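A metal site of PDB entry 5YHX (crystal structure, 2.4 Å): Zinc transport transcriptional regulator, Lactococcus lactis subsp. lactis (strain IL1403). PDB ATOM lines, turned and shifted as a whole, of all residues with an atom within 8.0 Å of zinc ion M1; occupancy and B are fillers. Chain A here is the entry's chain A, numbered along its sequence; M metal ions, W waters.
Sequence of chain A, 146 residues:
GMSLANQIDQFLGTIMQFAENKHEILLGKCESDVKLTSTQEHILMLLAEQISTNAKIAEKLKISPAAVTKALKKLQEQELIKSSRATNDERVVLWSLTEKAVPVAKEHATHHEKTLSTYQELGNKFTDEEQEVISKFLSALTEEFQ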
ATOM      1  N   LEU A  26      30.084  15.798 -25.795  1.00  0.00           N
ATOM      2  CA  LEU A  26      28.950  16.505 -25.206  1.00  0.00           C
ATOM      3  C   LEU A  26      29.417  17.901 -24.823  1.00  0.00           C
ATOM      4  O   LEU A  26      30.527  18.056 -24.322  1.00  0.00           O
ATOM      5  CB  LEU A  26      28.445  15.782 -23.961  1.00  0.00           C
ATOM      6  CG  LEU A  26      27.852  14.374 -24.142  1.00  0.00           C
ATOM      7  CD1 LEU A  26      27.680  13.703 -22.760  1.00  0.00           C
ATOM      8  CD2 LEU A  26      26.535  14.462 -24.894  1.00  0.00           C
ATOM      9  N   LYS A  29      28.719  21.150 -19.062  1.00  0.00           N
ATOM     10  CA  LYS A  29      29.096  20.234 -17.984  1.00  0.00           C
ATOM     11  C   LYS A  29      28.003  19.206 -17.727  1.00  0.00           C
ATOM     12  O   LYS A  29      26.819  19.532 -17.673  1.00  0.00           O
ATOM     13  CB  LYS A  29      29.335  21.005 -16.658  1.00  0.00           C
ATOM     14  CG  LYS A  29      30.384  22.131 -16.693  1.00  0.00           C
ATOM     15  CD  LYS A  29      30.716  22.642 -15.249  1.00  0.00           C
ATOM     16  CE  LYS A  29      31.822  23.732 -15.220  1.00  0.00           C
ATOM     17  NZ  LYS A  29      31.438  25.070 -15.840  1.00  0.00           N
ATOM     18  N   CYS A  30      28.404  17.950 -17.549  1.00  0.00           N
ATOM     19  CA  CYS A  30      27.485  16.984 -16.975  1.00  0.00           C
ATOM     20  C   CYS A  30      27.043  17.587 -15.654  1.00  0.00           C
ATOM     21  O   CYS A  30      27.893  18.061 -14.886  1.00  0.00           O
ATOM     22  CB  CYS A  30      28.195  15.665 -16.703  1.00  0.00           C
ATOM     23  SG  CYS A  30      27.240  14.529 -15.663  1.00  0.00           S
ATOM     24  N   GLU A  31      25.743  17.579 -15.393  1.00  0.00           N
ATOM     25  CA  GLU A  31      25.188  18.174 -14.177  1.00  0.00           C
ATOM     26  C   GLU A  31      24.594  17.105 -13.276  1.00  0.00           C
ATOM     27  O   GLU A  31      23.767  17.382 -12.414  1.00  0.00           O
ATOM     28  CB  GLU A  31      24.120  19.194 -14.520  1.00  0.00           C
ATOM     29  CG  GLU A  31      24.696  20.460 -15.149  1.00  0.00           C
ATOM     30  CD  GLU A  31      23.620  21.454 -15.585  1.00  0.00           C
ATOM     31  OE1 GLU A  31      22.406  21.199 -15.357  1.00  0.00           O
ATOM     32  OE2 GLU A  31      23.992  22.491 -16.163  1.00  0.00           O
ATOM     33  N   SER A  32      25.026  15.869 -13.498  1.00  0.00           N
ATOM     34  CA  SER A  32      24.564  14.767 -12.679  1.00  0.00           C
ATOM     35  C   SER A  32      25.278  14.783 -11.323  1.00  0.00           C
ATOM     36  O   SER A  32      26.491  15.052 -11.251  1.00  0.00           O
ATOM     37  CB  SER A  32      24.832  13.465 -13.417  1.00  0.00           C
ATOM     38  OG  SER A  32      24.062  12.420 -12.869  1.00  0.00           O
ATOM     39  N   ASP A  33      24.549  14.500 -10.247  1.00  0.00           N
ATOM     40  CA  ASP A  33      25.144  14.525  -8.892  1.00  0.00           C
ATOM     41  C   ASP A  33      25.899  13.235  -8.532  1.00  0.00           C
ATOM     42  O   ASP A  33      26.736  13.238  -7.637  1.00  0.00           O
ATOM     43  CB  ASP A  33      24.100  14.865  -7.826  1.00  0.00           C
ATOM     44  CG  ASP A  33      22.990  13.830  -7.733  1.00  0.00           C
ATOM     45  OD1 ASP A  33      22.814  13.042  -8.699  1.00  0.00           O
ATOM     46  OD2 ASP A  33      22.285  13.813  -6.688  1.00  0.00           O
ATOM     47  N   VAL A  34      25.581  12.147  -9.237  1.00  0.00           N
ATOM     48  CA  VAL A  34      26.307  10.900  -9.126  1.00  0.00           C
ATOM     49  C   VAL A  34      27.484  10.927 -10.096  1.00  0.00           C
ATOM     50  O   VAL A  34      27.309  11.165 -11.291  1.00  0.00           O
ATOM     51  CB  VAL A  34      25.383   9.699  -9.471  1.00  0.00           C
ATOM     52  CG1 VAL A  34      26.094   8.386  -9.212  1.00  0.00           C
ATOM     53  CG2 VAL A  34      24.075   9.769  -8.688  1.00  0.00           C
ATOM     54  N   LEU A  36      29.951   9.581 -12.538  1.00  0.00           N
ATOM     55  CA  LEU A  36      30.129   8.431 -13.433  1.00  0.00           C
ATOM     56  C   LEU A  36      30.792   8.885 -14.711  1.00  0.00           C
ATOM     57  O   LEU A  36      30.869  10.084 -14.984  1.00  0.00           O
ATOM     58  CB  LEU A  36      28.786   7.813 -13.774  1.00  0.00           C
ATOM     59  CG  LEU A  36      27.986   7.153 -12.661  1.00  0.00           C
ATOM     60  CD1 LEU A  36      26.598   6.812 -13.173  1.00  0.00           C
ATOM     61  CD2 LEU A  36      28.672   5.906 -12.124  1.00  0.00           C
ATOM     62  N   THR A  37      31.247   7.934 -15.525  1.00  0.00           N
ATOM     63  CA  THR A  37      31.856   8.248 -16.813  1.00  0.00           C
ATOM     64  C   THR A  37      30.774   8.491 -17.873  1.00  0.00           C
ATOM     65  O   THR A  37      29.653   7.992 -17.724  1.00  0.00           O
ATOM     66  CB  THR A  37      32.777   7.119 -17.291  1.00  0.00           C
ATOM     67  OG1 THR A  37      32.005   6.009 -17.750  1.00  0.00           O
ATOM     68  CG2 THR A  37      33.680   6.672 -16.144  1.00  0.00           C
ATOM     69  N   SER A  38      31.089   9.236 -18.933  1.00  0.00           N
ATOM     70  CA  SER A  38      30.148   9.392 -20.055  1.00  0.00           C
ATOM     71  C   SER A  38      29.574   8.042 -20.483  1.00  0.00           C
ATOM     72  O   SER A  38      28.369   7.902 -20.696  1.00  0.00           O
ATOM     73  CB  SER A  38      30.791  10.088 -21.251  1.00  0.00           C
ATOM     74  OG  SER A  38      31.817   9.285 -21.806  1.00  0.00           O
ATOM     75  N   GLU A  41      26.984   6.677 -17.858  1.00  0.00           N
ATOM     76  CA  GLU A  41      25.743   7.433 -17.891  1.00  0.00           C
ATOM     77  C   GLU A  41      24.997   7.127 -19.172  1.00  0.00           C
ATOM     78  O   GLU A  41      23.785   6.923 -19.164  1.00  0.00           O
ATOM     79  CB  GLU A  41      26.036   8.931 -17.805  1.00  0.00           C
ATOM     80  CG  GLU A  41      26.316   9.411 -16.402  1.00  0.00           C
ATOM     81  CD  GLU A  41      26.086  10.896 -16.252  1.00  0.00           C
ATOM     82  OE1 GLU A  41      25.514  11.505 -17.183  1.00  0.00           O
ATOM     83  OE2 GLU A  41      26.470  11.467 -15.203  1.00  0.00           O
ATOM     84  N   HIS A  42      25.749   7.044 -20.265  1.00  0.00           N
ATOM     85  CA  HIS A  42      25.148   6.676 -21.539  1.00  0.00           C
ATOM     86  C   HIS A  42      24.431   5.325 -21.491  1.00  0.00           C
ATOM     87  O   HIS A  42      23.356   5.192 -22.059  1.00  0.00           O
ATOM     88  CB  HIS A  42      26.176   6.695 -22.662  1.00  0.00           C
ATOM     89  CG  HIS A  42      25.552   6.732 -24.019  1.00  0.00           C
ATOM     90  ND1 HIS A  42      25.516   7.880 -24.782  1.00  0.00           N
ATOM     91  CD2 HIS A  42      24.884   5.787 -24.723  1.00  0.00           C
ATOM     92  CE1 HIS A  42      24.893   7.634 -25.917  1.00  0.00           C
ATOM     93  NE2 HIS A  42      24.492   6.365 -25.900  1.00  0.00           N
ATOM     94  N   PRO A 103      16.900   9.688 -12.503  1.00  0.00           N
ATOM     95  CA  PRO A 103      17.324  11.075 -12.745  1.00  0.00           C
ATOM     96  C   PRO A 103      18.656  11.134 -13.494  1.00  0.00           C
ATOM     97  O   PRO A 103      18.900  12.098 -14.218  1.00  0.00           O
ATOM     98  CB  PRO A 103      17.524  11.641 -11.334  1.00  0.00           C
ATOM     99  CG  PRO A 103      16.905  10.656 -10.408  1.00  0.00           C
ATOM    100  CD  PRO A 103      16.957   9.325 -11.083  1.00  0.00           C
ATOM    101  N   VAL A 104      19.514  10.142 -13.296  1.00  0.00           N
ATOM    102  CA  VAL A 104      20.805  10.167 -13.977  1.00  0.00           C
ATOM    103  C   VAL A 104      20.647   9.924 -15.477  1.00  0.00           C
ATOM    104  O   VAL A 104      21.212  10.651 -16.290  1.00  0.00           O
ATOM    105  CB  VAL A 104      21.788   9.154 -13.396  1.00  0.00           C
ATOM    106  CG1 VAL A 104      23.098   9.181 -14.186  1.00  0.00           C
ATOM    107  CG2 VAL A 104      22.030   9.436 -11.920  1.00  0.00           C
ATOM    108  N   ALA A 105      19.851   8.917 -15.853  1.00  0.00           N
ATOM    109  CA  ALA A 105      19.510   8.695 -17.256  1.00  0.00           C
ATOM    110  C   ALA A 105      18.943   9.978 -17.809  1.00  0.00           C
ATOM    111  O   ALA A 105      19.363  10.466 -18.868  1.00  0.00           O
ATOM    112  CB  ALA A 105      18.500   7.579 -17.428  1.00  0.00           C
ATOM    113  N   LYS A 106      17.997  10.524 -17.055  1.00  0.00           N
ATOM    114  CA  LYS A 106      17.289  11.704 -17.492  1.00  0.00           C
ATOM    115  C   LYS A 106      18.267  12.838 -17.732  1.00  0.00           C
ATOM    116  O   LYS A 106      18.189  13.528 -18.744  1.00  0.00           O
ATOM    117  CB  LYS A 106      16.184  12.073 -16.501  1.00  0.00           C
ATOM    118  CG  LYS A 106      15.391  13.338 -16.860  1.00  0.00           C
ATOM    119  CD  LYS A 106      14.181  13.543 -15.933  1.00  0.00           C
ATOM    120  CE  LYS A 106      13.335  12.267 -15.837  1.00  0.00           C
ATOM    121  NZ  LYS A 106      12.853  11.782 -17.173  1.00  0.00           N
ATOM    122  N   GLU A 107      19.226  13.040 -16.834  1.00  0.00           N
ATOM    123  CA  GLU A 107      20.114  14.187 -16.993  1.00  0.00           C
ATOM    124  C   GLU A 107      20.994  14.044 -18.237  1.00  0.00           C
ATOM    125  O   GLU A 107      21.214  14.999 -18.982  1.00  0.00           O
ATOM    126  CB  GLU A 107      20.984  14.398 -15.746  1.00  0.00           C
ATOM    127  CG  GLU A 107      21.970  15.562 -15.852  1.00  0.00           C
ATOM    128  CD  GLU A 107      23.236  15.197 -16.579  1.00  0.00           C
ATOM    129  OE1 GLU A 107      23.572  13.991 -16.616  1.00  0.00           O
ATOM    130  OE2 GLU A 107      23.896  16.107 -17.113  1.00  0.00           O
ATOM    131  N   HIS A 108      21.488  12.826 -18.454  1.00  0.00           N
ATOM    132  CA  HIS A 108      22.373  12.548 -19.584  1.00  0.00           C
ATOM    133  C   HIS A 108      21.679  12.719 -20.931  1.00  0.00           C
ATOM    134  O   HIS A 108      22.249  13.271 -21.879  1.00  0.00           O
ATOM    135  CB  HIS A 108      22.927  11.133 -19.478  1.00  0.00           C
ATOM    136  CG  HIS A 108      24.079  10.874 -20.379  1.00  0.00           C
ATOM    137  ND1 HIS A 108      25.261  11.601 -20.292  1.00  0.00           N
ATOM    138  CD2 HIS A 108      24.246  10.016 -21.405  1.00  0.00           C
ATOM    139  CE1 HIS A 108      26.091  11.176 -21.228  1.00  0.00           C
ATOM    140  NE2 HIS A 108      25.504  10.207 -21.901  1.00  0.00           N
ATOM    141  N   ALA A 109      20.428  12.246 -21.013  1.00  0.00           N
ATOM    142  CA  ALA A 109      19.585  12.499 -22.199  1.00  0.00           C
ATOM    143  C   ALA A 109      19.487  13.995 -22.458  1.00  0.00           C
ATOM    144  O   ALA A 109      19.601  14.463 -23.603  1.00  0.00           O
ATOM    145  CB  ALA A 109      18.190  11.914 -22.003  1.00  0.00           C
ATOM    146  N   THR A 110      19.287  14.733 -21.374  1.00  0.00           N
ATOM    147  CA  THR A 110      19.194  16.186 -21.472  1.00  0.00           C
ATOM    148  C   THR A 110      20.517  16.758 -21.971  1.00  0.00           C
ATOM    149  O   THR A 110      20.549  17.625 -22.825  1.00  0.00           O
ATOM    150  CB  THR A 110      18.810  16.803 -20.117  1.00  0.00           C
ATOM    151  OG1 THR A 110      17.508  16.326 -19.751  1.00  0.00           O
ATOM    152  CG2 THR A 110      18.801  18.323 -20.154  1.00  0.00           C
ATOM    153  N   HIS A 111      21.612  16.258 -21.420  1.00  0.00           N
ATOM    154  CA  HIS A 111      22.914  16.723 -21.855  1.00  0.00           C
ATOM    155  C   HIS A 111      23.009  16.515 -23.382  1.00  0.00           C
ATOM    156  O   HIS A 111      23.454  17.390 -24.125  1.00  0.00           O
ATOM    157  CB  HIS A 111      24.011  15.969 -21.091  1.00  0.00           C
ATOM    158  CG  HIS A 111      25.327  16.678 -21.070  1.00  0.00           C
ATOM    159  ND1 HIS A 111      26.356  16.317 -20.230  1.00  0.00           N
ATOM    160  CD2 HIS A 111      25.800  17.715 -21.818  1.00  0.00           C
ATOM    161  CE1 HIS A 111      27.404  17.102 -20.445  1.00  0.00           C
ATOM    162  NE2 HIS A 111      27.088  17.955 -21.401  1.00  0.00           N
ATOM    163  N   HIS A 112      22.551  15.362 -23.856  1.00  0.00           N
ATOM    164  CA  HIS A 112      22.449  15.163 -25.315  1.00  0.00           C
ATOM    165  C   HIS A 112      21.579  16.206 -26.003  1.00  0.00           C
ATOM    166  O   HIS A 112      21.965  16.782 -27.026  1.00  0.00           O
ATOM    167  CB  HIS A 112      22.013  13.737 -25.664  1.00  0.00           C
ATOM    168  CG  HIS A 112      23.154  12.790 -25.732  1.00  0.00           C
ATOM    169  ND1 HIS A 112      24.028  12.766 -26.797  1.00  0.00           N
ATOM    170  CD2 HIS A 112      23.647  11.914 -24.827  1.00  0.00           C
ATOM    171  CE1 HIS A 112      24.973  11.881 -26.573  1.00  0.00           C
ATOM    172  NE2 HIS A 112      24.770  11.348 -25.377  1.00  0.00           N
HETATM  173 ZN    ZN M   1      25.641  13.509 -17.128  1.00  0.00          ZN
HETATM  174 ZN    ZN M   2      25.794   9.832 -24.144  1.00  0.00          ZN
HETATM  175  O   HOH W   1      26.196  14.337 -18.651  1.00  0.00           O
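Water W1 binds zinc ion M1 (1.8 Å).
OE1 of Glu 41 is bound to zinc ion M1, 2.0 Å away.
Zinc ion M1 is bound by OE1 of Glu 107 (2.2 Å).
Zinc ion M1 is bound by SG of Cys 30 (2.4 Å).
The side-chain carboxylate (OE1) of Glu 41 lies close to a ring nitrogen (ND1) of His 108 (3.1 Å).
The side-chain carboxylate (OE2) of Glu 41 sits close to the side-chain hydroxyl (OG) of Ser 32.
The backbone NH (N) of Glu 31 lies within hydrogen-bond range of the side-chain carboxylate (OE2) of Glu 107, 2.9 Å away.
SG of Cys 30 sits close to N of Ser 32 (3.4 Å).
Residues that only touch zinc ion M1: Ser 32 and His 108.
Five residues have an atom within 4 Å of zinc ion M1: Cys 30, Ser 32, Glu 41, Glu 107 and His 108.
Water W1 lies within hydrogen-bond range of a ring nitrogen (ND1) of His 111, the side-chain carboxylate of Glu 107 and a ring nitrogen (ND1) of His 108.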
